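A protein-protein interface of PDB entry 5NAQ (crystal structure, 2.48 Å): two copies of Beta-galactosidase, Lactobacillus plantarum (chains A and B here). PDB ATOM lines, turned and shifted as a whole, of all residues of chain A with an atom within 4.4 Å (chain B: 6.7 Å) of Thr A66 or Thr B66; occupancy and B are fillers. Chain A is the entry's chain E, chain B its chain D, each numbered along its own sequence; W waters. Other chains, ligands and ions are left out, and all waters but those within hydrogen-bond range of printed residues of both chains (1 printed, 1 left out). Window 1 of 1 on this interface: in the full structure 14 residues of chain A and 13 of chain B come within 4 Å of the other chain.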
ATOM      1  N   THR A  35     -15.959  -8.656 -37.591  1.00  0.00           N
ATOM      2  CA  THR A  35     -16.315  -7.275 -37.246  1.00  0.00           C
ATOM      3  C   THR A  35     -17.727  -7.110 -36.706  1.00  0.00           C
ATOM      4  O   THR A  35     -17.938  -6.275 -35.817  1.00  0.00           O
ATOM      5  CB  THR A  35     -16.154  -6.344 -38.477  1.00  0.00           C
ATOM      6  OG1 THR A  35     -16.957  -6.844 -39.553  1.00  0.00           O
ATOM      7  CG2 THR A  35     -14.700  -6.282 -38.911  1.00  0.00           C
ATOM      8  N   GLU A  36     -18.704  -7.866 -37.231  1.00  0.00           N
ATOM      9  CA  GLU A  36     -20.096  -7.446 -37.082  1.00  0.00           C
ATOM     10  C   GLU A  36     -20.683  -7.780 -35.723  1.00  0.00           C
ATOM     11  O   GLU A  36     -21.488  -7.001 -35.203  1.00  0.00           O
ATOM     12  CB  GLU A  36     -20.986  -8.053 -38.172  1.00  0.00           C
ATOM     13  CG  GLU A  36     -20.449  -7.958 -39.571  1.00  0.00           C
ATOM     14  CD  GLU A  36     -21.160  -8.907 -40.538  1.00  0.00           C
ATOM     15  OE1 GLU A  36     -20.927  -8.801 -41.753  1.00  0.00           O
ATOM     16  OE2 GLU A  36     -21.966  -9.752 -40.112  1.00  0.00           O
ATOM     17  N   GLY A  37     -20.282  -8.893 -35.130  1.00  0.00           N
ATOM     18  CA  GLY A  37     -21.063  -9.499 -34.081  1.00  0.00           C
ATOM     19  C   GLY A  37     -22.066 -10.477 -34.668  1.00  0.00           C
ATOM     20  O   GLY A  37     -22.348 -10.485 -35.866  1.00  0.00           O
ATOM     21  N   PHE A  39     -25.184 -10.589 -33.844  1.00  0.00           N
ATOM     22  CA  PHE A  39     -26.508 -10.021 -33.655  1.00  0.00           C
ATOM     23  C   PHE A  39     -27.465 -10.471 -34.750  1.00  0.00           C
ATOM     24  O   PHE A  39     -27.219 -10.253 -35.942  1.00  0.00           O
ATOM     25  CB  PHE A  39     -26.417  -8.494 -33.640  1.00  0.00           C
ATOM     26  CG  PHE A  39     -25.419  -7.947 -32.667  1.00  0.00           C
ATOM     27  CD1 PHE A  39     -24.111  -7.707 -33.053  1.00  0.00           C
ATOM     28  CD2 PHE A  39     -25.802  -7.644 -31.369  1.00  0.00           C
ATOM     29  CE1 PHE A  39     -23.199  -7.199 -32.158  1.00  0.00           C
ATOM     30  CE2 PHE A  39     -24.901  -7.134 -30.470  1.00  0.00           C
ATOM     31  CZ  PHE A  39     -23.594  -6.908 -30.861  1.00  0.00           C
ATOM     32  N   PRO A  64     -16.791 -14.190 -31.135  1.00  0.00           N
ATOM     33  CA  PRO A  64     -17.281 -13.332 -32.219  1.00  0.00           C
ATOM     34  C   PRO A  64     -18.687 -12.783 -32.015  1.00  0.00           C
ATOM     35  O   PRO A  64     -19.192 -12.068 -32.894  1.00  0.00           O
ATOM     36  CB  PRO A  64     -17.239 -14.290 -33.420  1.00  0.00           C
ATOM     37  CG  PRO A  64     -17.606 -15.621 -32.823  1.00  0.00           C
ATOM     38  CD  PRO A  64     -17.097 -15.608 -31.376  1.00  0.00           C
ATOM     39  N   ASP A  65     -19.318 -13.085 -30.877  1.00  0.00           N
ATOM     40  CA  ASP A  65     -20.725 -12.743 -30.690  1.00  0.00           C
ATOM     41  C   ASP A  65     -20.952 -11.234 -30.700  1.00  0.00           C
ATOM     42  O   ASP A  65     -22.022 -10.779 -31.120  1.00  0.00           O
ATOM     43  CB  ASP A  65     -21.257 -13.361 -29.387  1.00  0.00           C
ATOM     44  CG  ASP A  65     -21.240 -14.901 -29.399  1.00  0.00           C
ATOM     45  OD1 ASP A  65     -21.128 -15.525 -30.486  1.00  0.00           O
ATOM     46  OD2 ASP A  65     -21.355 -15.491 -28.303  1.00  0.00           O
ATOM     47  N   THR A  66     -19.975 -10.443 -30.248  1.00  0.00           N
ATOM     48  CA  THR A  66     -20.039  -8.989 -30.401  1.00  0.00           C
ATOM     49  C   THR A  66     -19.012  -8.462 -31.390  1.00  0.00           C
ATOM     50  O   THR A  66     -19.332  -7.586 -32.189  1.00  0.00           O
ATOM     51  CB  THR A  66     -19.867  -8.282 -29.039  1.00  0.00           C
ATOM     52  OG1 THR A  66     -21.055  -8.447 -28.255  1.00  0.00           O
ATOM     53  CG2 THR A  66     -19.642  -6.804 -29.201  1.00  0.00           C
ATOM     54  N   ALA A  67     -17.811  -9.044 -31.400  1.00  0.00           N
ATOM     55  CA  ALA A  67     -16.670  -8.651 -32.255  1.00  0.00           C
ATOM     56  C   ALA A  67     -16.469  -7.147 -32.098  1.00  0.00           C
ATOM     57  O   ALA A  67     -16.330  -6.672 -30.961  1.00  0.00           O
ATOM     58  CB  ALA A  67     -16.865  -9.127 -33.695  1.00  0.00           C
ATOM     59  N   SER A  68     -16.435  -6.380 -33.186  1.00  0.00           N
ATOM     60  CA  SER A  68     -16.246  -4.938 -33.159  1.00  0.00           C
ATOM     61  C   SER A  68     -17.546  -4.186 -33.414  1.00  0.00           C
ATOM     62  O   SER A  68     -17.521  -3.010 -33.787  1.00  0.00           O
ATOM     63  CB  SER A  68     -15.175  -4.547 -34.174  1.00  0.00           C
ATOM     64  OG  SER A  68     -13.911  -5.024 -33.753  1.00  0.00           O
ATOM     65  N   ASN A  69     -18.681  -4.856 -33.224  1.00  0.00           N
ATOM     66  CA  ASN A  69     -19.987  -4.207 -33.114  1.00  0.00           C
ATOM     67  C   ASN A  69     -20.375  -3.498 -34.410  1.00  0.00           C
ATOM     68  O   ASN A  69     -21.156  -2.538 -34.405  1.00  0.00           O
ATOM     69  CB  ASN A  69     -20.007  -3.249 -31.913  1.00  0.00           C
ATOM     70  CG  ASN A  69     -21.404  -2.892 -31.472  1.00  0.00           C
ATOM     71  OD1 ASN A  69     -22.300  -3.753 -31.429  1.00  0.00           O
ATOM     72  ND2 ASN A  69     -21.594  -1.625 -31.074  1.00  0.00           N
ATOM     73  N   GLN A 457     -16.923  -0.747 -26.975  1.00  0.00           N
ATOM     74  CA  GLN A 457     -17.063  -0.594 -28.426  1.00  0.00           C
ATOM     75  C   GLN A 457     -16.890   0.868 -28.854  1.00  0.00           C
ATOM     76  O   GLN A 457     -17.580   1.371 -29.744  1.00  0.00           O
ATOM     77  CB  GLN A 457     -18.401  -1.165 -28.911  1.00  0.00           C
ATOM     78  CG  GLN A 457     -18.533  -2.656 -28.673  1.00  0.00           C
ATOM     79  CD  GLN A 457     -17.534  -3.467 -29.486  1.00  0.00           C
ATOM     80  OE1 GLN A 457     -17.091  -3.035 -30.557  1.00  0.00           O
ATOM     81  NE2 GLN A 457     -17.159  -4.642 -28.973  1.00  0.00           N
ATOM     82  N   GLN B  34     -27.487  -4.916 -15.901  1.00  0.00           N
ATOM     83  CA  GLN B  34     -27.746  -6.303 -16.267  1.00  0.00           C
ATOM     84  C   GLN B  34     -28.371  -6.440 -17.649  1.00  0.00           C
ATOM     85  O   GLN B  34     -28.524  -7.567 -18.124  1.00  0.00           O
ATOM     86  CB  GLN B  34     -28.631  -6.981 -15.198  1.00  0.00           C
ATOM     87  CG  GLN B  34     -28.020  -6.852 -13.810  1.00  0.00           C
ATOM     88  CD  GLN B  34     -28.871  -7.402 -12.688  1.00  0.00           C
ATOM     89  OE1 GLN B  34     -29.623  -6.663 -12.046  1.00  0.00           O
ATOM     90  NE2 GLN B  34     -28.718  -8.692 -12.403  1.00  0.00           N
ATOM     91  N   THR B  35     -28.705  -5.323 -18.329  1.00  0.00           N
ATOM     92  CA  THR B  35     -29.385  -5.430 -19.622  1.00  0.00           C
ATOM     93  C   THR B  35     -28.700  -4.688 -20.765  1.00  0.00           C
ATOM     94  O   THR B  35     -28.607  -5.237 -21.865  1.00  0.00           O
ATOM     95  CB  THR B  35     -30.831  -4.921 -19.504  1.00  0.00           C
ATOM     96  OG1 THR B  35     -30.829  -3.575 -19.023  1.00  0.00           O
ATOM     97  CG2 THR B  35     -31.635  -5.784 -18.573  1.00  0.00           C
ATOM     98  N   GLU B  36     -28.207  -3.468 -20.531  1.00  0.00           N
ATOM     99  CA  GLU B  36     -27.878  -2.553 -21.625  1.00  0.00           C
ATOM    100  C   GLU B  36     -26.717  -3.056 -22.477  1.00  0.00           C
ATOM    101  O   GLU B  36     -26.770  -2.984 -23.710  1.00  0.00           O
ATOM    102  CB  GLU B  36     -27.525  -1.176 -21.061  1.00  0.00           C
ATOM    103  CG  GLU B  36     -28.682  -0.369 -20.529  1.00  0.00           C
ATOM    104  CD  GLU B  36     -28.223   0.748 -19.643  1.00  0.00           C
ATOM    105  OE1 GLU B  36     -27.006   1.018 -19.641  1.00  0.00           O
ATOM    106  OE2 GLU B  36     -29.071   1.346 -18.943  1.00  0.00           O
ATOM    107  N   GLY B  37     -25.662  -3.550 -21.838  1.00  0.00           N
ATOM    108  CA  GLY B  37     -24.340  -3.549 -22.422  1.00  0.00           C
ATOM    109  C   GLY B  37     -23.610  -2.255 -22.087  1.00  0.00           C
ATOM    110  O   GLY B  37     -24.186  -1.274 -21.626  1.00  0.00           O
ATOM    111  N   ASN B  38     -22.301  -2.263 -22.300  1.00  0.00           N
ATOM    112  CA  ASN B  38     -21.453  -1.107 -22.041  1.00  0.00           C
ATOM    113  C   ASN B  38     -21.243  -0.255 -23.287  1.00  0.00           C
ATOM    114  O   ASN B  38     -20.278   0.518 -23.351  1.00  0.00           O
ATOM    115  CB  ASN B  38     -20.105  -1.570 -21.490  1.00  0.00           C
ATOM    116  CG  ASN B  38     -20.191  -2.017 -20.044  1.00  0.00           C
ATOM    117  OD1 ASN B  38     -20.956  -1.447 -19.257  1.00  0.00           O
ATOM    118  ND2 ASN B  38     -19.395  -3.027 -19.680  1.00  0.00           N
ATOM    119  N   PHE B  39     -22.109  -0.408 -24.283  1.00  0.00           N
ATOM    120  CA  PHE B  39     -21.945   0.291 -25.549  1.00  0.00           C
ATOM    121  C   PHE B  39     -21.851   1.790 -25.305  1.00  0.00           C
ATOM    122  O   PHE B  39     -22.776   2.396 -24.757  1.00  0.00           O
ATOM    123  CB  PHE B  39     -23.106  -0.042 -26.494  1.00  0.00           C
ATOM    124  CG  PHE B  39     -23.208  -1.508 -26.817  1.00  0.00           C
ATOM    125  CD1 PHE B  39     -24.079  -2.329 -26.116  1.00  0.00           C
ATOM    126  CD2 PHE B  39     -22.392  -2.072 -27.794  1.00  0.00           C
ATOM    127  CE1 PHE B  39     -24.148  -3.674 -26.387  1.00  0.00           C
ATOM    128  CE2 PHE B  39     -22.453  -3.410 -28.076  1.00  0.00           C
ATOM    129  CZ  PHE B  39     -23.334  -4.219 -27.378  1.00  0.00           C
ATOM    130  N   GLY B  63     -19.323 -11.262 -19.321  1.00  0.00           N
ATOM    131  CA  GLY B  63     -19.460 -10.085 -18.506  1.00  0.00           C
ATOM    132  C   GLY B  63     -20.616  -9.206 -18.948  1.00  0.00           C
ATOM    133  O   GLY B  63     -21.533  -9.632 -19.659  1.00  0.00           O
ATOM    134  N   PRO B  64     -20.592  -7.947 -18.520  1.00  0.00           N
ATOM    135  CA  PRO B  64     -21.698  -7.031 -18.813  1.00  0.00           C
ATOM    136  C   PRO B  64     -21.547  -6.208 -20.087  1.00  0.00           C
ATOM    137  O   PRO B  64     -22.417  -5.365 -20.341  1.00  0.00           O
ATOM    138  CB  PRO B  64     -21.688  -6.123 -17.571  1.00  0.00           C
ATOM    139  CG  PRO B  64     -20.204  -6.000 -17.258  1.00  0.00           C
ATOM    140  CD  PRO B  64     -19.584  -7.345 -17.629  1.00  0.00           C
ATOM    141  N   ASP B  65     -20.506  -6.437 -20.907  1.00  0.00           N
ATOM    142  CA  ASP B  65     -20.240  -5.543 -22.036  1.00  0.00           C
ATOM    143  C   ASP B  65     -21.314  -5.617 -23.111  1.00  0.00           C
ATOM    144  O   ASP B  65     -21.487  -4.657 -23.875  1.00  0.00           O
ATOM    145  CB  ASP B  65     -18.859  -5.811 -22.654  1.00  0.00           C
ATOM    146  CG  ASP B  65     -17.740  -5.779 -21.626  1.00  0.00           C
ATOM    147  OD1 ASP B  65     -17.915  -5.112 -20.578  1.00  0.00           O
ATOM    148  OD2 ASP B  65     -16.648  -6.320 -21.900  1.00  0.00           O
ATOM    149  N   THR B  66     -22.031  -6.722 -23.204  1.00  0.00           N
ATOM    150  CA  THR B  66     -23.169  -6.784 -24.118  1.00  0.00           C
ATOM    151  C   THR B  66     -24.470  -7.069 -23.392  1.00  0.00           C
ATOM    152  O   THR B  66     -25.521  -6.533 -23.773  1.00  0.00           O
ATOM    153  CB  THR B  66     -22.930  -7.859 -25.214  1.00  0.00           C
ATOM    154  OG1 THR B  66     -21.780  -7.520 -26.002  1.00  0.00           O
ATOM    155  CG2 THR B  66     -24.127  -7.991 -26.136  1.00  0.00           C
ATOM    156  N   ALA B  67     -24.408  -7.884 -22.333  1.00  0.00           N
ATOM    157  CA  ALA B  67     -25.573  -8.302 -21.570  1.00  0.00           C
ATOM    158  C   ALA B  67     -26.672  -8.768 -22.511  1.00  0.00           C
ATOM    159  O   ALA B  67     -26.459  -9.651 -23.349  1.00  0.00           O
ATOM    160  CB  ALA B  67     -26.070  -7.163 -20.670  1.00  0.00           C
ATOM    161  N   SER B  68     -27.849  -8.157 -22.380  1.00  0.00           N
ATOM    162  CA  SER B  68     -28.993  -8.468 -23.221  1.00  0.00           C
ATOM    163  C   SER B  68     -29.222  -7.404 -24.283  1.00  0.00           C
ATOM    164  O   SER B  68     -30.349  -7.228 -24.759  1.00  0.00           O
ATOM    165  CB  SER B  68     -30.230  -8.669 -22.347  1.00  0.00           C
ATOM    166  OG  SER B  68     -30.072  -9.849 -21.553  1.00  0.00           O
ATOM    167  N   ASN B  69     -28.163  -6.673 -24.645  1.00  0.00           N
ATOM    168  CA  ASN B  69     -28.138  -5.817 -25.820  1.00  0.00           C
ATOM    169  C   ASN B  69     -29.186  -4.711 -25.756  1.00  0.00           C
ATOM    170  O   ASN B  69     -29.573  -4.147 -26.798  1.00  0.00           O
ATOM    171  CB  ASN B  69     -28.304  -6.665 -27.094  1.00  0.00           C
ATOM    172  CG  ASN B  69     -27.951  -5.903 -28.373  1.00  0.00           C
ATOM    173  OD1 ASN B  69     -27.013  -5.111 -28.396  1.00  0.00           O
ATOM    174  ND2 ASN B  69     -28.715  -6.139 -29.439  1.00  0.00           N
ATOM    175  N   PHE B  70     -29.653  -4.361 -24.550  1.00  0.00           N
ATOM    176  CA  PHE B  70     -30.768  -3.415 -24.444  1.00  0.00           C
ATOM    177  C   PHE B  70     -30.399  -2.030 -24.953  1.00  0.00           C
ATOM    178  O   PHE B  70     -31.288  -1.280 -25.372  1.00  0.00           O
ATOM    179  CB  PHE B  70     -31.267  -3.298 -23.005  1.00  0.00           C
ATOM    180  CG  PHE B  70     -32.640  -2.666 -22.878  1.00  0.00           C
ATOM    181  CD1 PHE B  70     -32.829  -1.471 -22.182  1.00  0.00           C
ATOM    182  CD2 PHE B  70     -33.745  -3.270 -23.457  1.00  0.00           C
ATOM    183  CE1 PHE B  70     -34.110  -0.905 -22.055  1.00  0.00           C
ATOM    184  CE2 PHE B  70     -35.020  -2.715 -23.338  1.00  0.00           C
ATOM    185  CZ  PHE B  70     -35.203  -1.538 -22.641  1.00  0.00           C
ATOM    186  N   TYR B  71     -29.113  -1.660 -24.909  1.00  0.00           N
ATOM    187  CA  TYR B  71     -28.705  -0.375 -25.477  1.00  0.00           C
ATOM    188  C   TYR B  71     -29.070  -0.275 -26.951  1.00  0.00           C
ATOM    189  O   TYR B  71     -29.490   0.788 -27.418  1.00  0.00           O
ATOM    190  CB  TYR B  71     -27.211  -0.156 -25.294  1.00  0.00           C
ATOM    191  CG  TYR B  71     -26.687   1.138 -25.889  1.00  0.00           C
ATOM    192  CD1 TYR B  71     -26.642   2.301 -25.135  1.00  0.00           C
ATOM    193  CD2 TYR B  71     -26.227   1.192 -27.192  1.00  0.00           C
ATOM    194  CE1 TYR B  71     -26.150   3.478 -25.660  1.00  0.00           C
ATOM    195  CE2 TYR B  71     -25.722   2.356 -27.727  1.00  0.00           C
ATOM    196  CZ  TYR B  71     -25.691   3.503 -26.957  1.00  0.00           C
ATOM    197  OH  TYR B  71     -25.202   4.679 -27.473  1.00  0.00           O
ATOM    198  N   ASN B  72     -28.923  -1.367 -27.698  1.00  0.00           N
ATOM    199  CA  ASN B  72     -29.246  -1.339 -29.117  1.00  0.00           C
ATOM    200  C   ASN B  72     -30.692  -1.707 -29.431  1.00  0.00           C
ATOM    201  O   ASN B  72     -31.235  -1.234 -30.430  1.00  0.00           O
ATOM    202  CB  ASN B  72     -28.333  -2.299 -29.888  1.00  0.00           C
ATOM    203  CG  ASN B  72     -26.923  -1.806 -29.984  1.00  0.00           C
ATOM    204  OD1 ASN B  72     -26.670  -0.743 -30.562  1.00  0.00           O
ATOM    205  ND2 ASN B  72     -25.977  -2.580 -29.433  1.00  0.00           N
ATOM    206  N   TYR B 443     -25.231 -15.553 -17.044  1.00  0.00           N
ATOM    207  CA  TYR B 443     -26.406 -16.156 -17.668  1.00  0.00           C
ATOM    208  C   TYR B 443     -26.575 -17.638 -17.310  1.00  0.00           C
ATOM    209  O   TYR B 443     -27.231 -18.381 -18.049  1.00  0.00           O
ATOM    210  CB  TYR B 443     -26.349 -15.950 -19.188  1.00  0.00           C
ATOM    211  CG  TYR B 443     -26.684 -14.526 -19.545  1.00  0.00           C
ATOM    212  CD1 TYR B 443     -28.003 -14.120 -19.674  1.00  0.00           C
ATOM    213  CD2 TYR B 443     -25.685 -13.569 -19.705  1.00  0.00           C
ATOM    214  CE1 TYR B 443     -28.317 -12.814 -19.969  1.00  0.00           C
ATOM    215  CE2 TYR B 443     -25.994 -12.259 -19.997  1.00  0.00           C
ATOM    216  CZ  TYR B 443     -27.306 -11.893 -20.126  1.00  0.00           C
ATOM    217  OH  TYR B 443     -27.619 -10.593 -20.410  1.00  0.00           O
ATOM    218  N   ILE B 454     -27.923 -15.524 -26.041  1.00  0.00           N
ATOM    219  CA  ILE B 454     -26.991 -14.406 -25.920  1.00  0.00           C
ATOM    220  C   ILE B 454     -25.895 -14.424 -26.971  1.00  0.00           C
ATOM    221  O   ILE B 454     -25.109 -13.470 -27.047  1.00  0.00           O
ATOM    222  CB  ILE B 454     -26.371 -14.386 -24.513  1.00  0.00           C
ATOM    223  CG1 ILE B 454     -25.476 -15.595 -24.314  1.00  0.00           C
ATOM    224  CG2 ILE B 454     -27.451 -14.424 -23.450  1.00  0.00           C
ATOM    225  CD1 ILE B 454     -24.778 -15.576 -22.984  1.00  0.00           C
ATOM    226  N   HIS B 455     -25.806 -15.479 -27.784  1.00  0.00           N
ATOM    227  CA  HIS B 455     -24.886 -15.441 -28.919  1.00  0.00           C
ATOM    228  C   HIS B 455     -25.414 -14.519 -30.006  1.00  0.00           C
ATOM    229  O   HIS B 455     -24.682 -13.663 -30.510  1.00  0.00           O
ATOM    230  CB  HIS B 455     -24.646 -16.847 -29.468  1.00  0.00           C
ATOM    231  CG  HIS B 455     -24.106 -17.785 -28.445  1.00  0.00           C
ATOM    232  ND1 HIS B 455     -22.923 -17.545 -27.772  1.00  0.00           N
ATOM    233  CD2 HIS B 455     -24.605 -18.941 -27.942  1.00  0.00           C
ATOM    234  CE1 HIS B 455     -22.703 -18.529 -26.918  1.00  0.00           C
ATOM    235  NE2 HIS B 455     -23.710 -19.386 -26.997  1.00  0.00           N
ATOM    236  N   GLN B 457     -28.337 -12.594 -29.549  1.00  0.00           N
ATOM    237  CA  GLN B 457     -29.271 -11.627 -28.953  1.00  0.00           C
ATOM    238  C   GLN B 457     -30.664 -11.762 -29.560  1.00  0.00           C
ATOM    239  O   GLN B 457     -31.397 -10.788 -29.724  1.00  0.00           O
ATOM    240  CB  GLN B 457     -28.746 -10.192 -29.069  1.00  0.00           C
ATOM    241  CG  GLN B 457     -27.523  -9.937 -28.183  1.00  0.00           C
ATOM    242  CD  GLN B 457     -27.812 -10.146 -26.698  1.00  0.00           C
ATOM    243  OE1 GLN B 457     -28.900  -9.831 -26.201  1.00  0.00           O
ATOM    244  NE2 GLN B 457     -26.815 -10.661 -25.973  1.00  0.00           N
HETATM  245  O   HOH W   1     -23.902   0.074 -30.726  1.00  0.00           O
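Water W1 lies within hydrogen-bond range of ND2 of Asn A69 (2.9 Å) and OD1 of Asn B72 (2.9 Å).
Among the printed residues, merely in contact across the chains: Phe A39 with Asn B69 and Asn A69 with Phe B39.
Printed residues of chain B within 4 Å of Phe A39: Asn B69 (3.6 Å). Of the printed residues of chain B, Asp A65 touches His B455 (2.6 Å). Of the printed residues of chain B, Asn A69 touches Phe B39. Asn B38 touches none of the printed residues of chain A. Of the printed residues of chain A, Phe B39 touches Asn A69. Gly B63 touches none of the printed residues of chain A. Of chain A, only Thr A66 (2.5 Å) comes within 4 Å of Thr B66. Printed residues of chain A within 4 Å of His B455: Asp A65 (2.6 Å). The nearest printed residue of chain A that does not touch His B455 is Phe A39 (4.6 Å).
Phe A39 touches Asn B69, and with the chains exchanged Asn A69 touches Phe B39. Thr A66 touches its own counterpart, Thr B66. Positions printed for both chains: 35, 36, 37, 39, 64, 65, 66, 67, 68, 69 and 457. Of the 4 pairs that touch across the chains among the printed residues, 3 have their exchanged pair printed and touching as well.
Of the 11 printed residues of chain A, 4 touch a printed residue of chain B. Hydrophobic or aromatic side chains of chain B within 4 Å of the printed part of chain A: Phe B39 and His B455. Along chain B the printed residues that touch a printed residue of chain A span positions 39 to 455. Among the printed residues, no Asp or Glu carboxylate lies within 4 Å of a Lys or Arg side-chain nitrogen of the other chain.
The backbone NH of Asn B69 sits at hydrogen-bond distance from the backbone carbonyl oxygen of Thr B35 (3.2 Å). OD1 of Asn B69 sits at hydrogen-bond distance from ND2 of Asn B72 (2.9 Å). The backbone NH (N) of Asn A69 is in hydrogen-bond range of the backbone carbonyl oxygen (O) of Thr A35. The backbone carbonyl oxygen (O) of Thr A66 lies close to the backbone NH (N) of Gly A37, 3.4 Å away.
The side-chain hydroxyl of Thr A66 is in hydrogen-bond range of the side-chain hydroxyl of Thr B66, at 2.5 Å. ND1 of His B455 is in hydrogen-bond range of OD2 of Asp A65 (2.6 Å).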
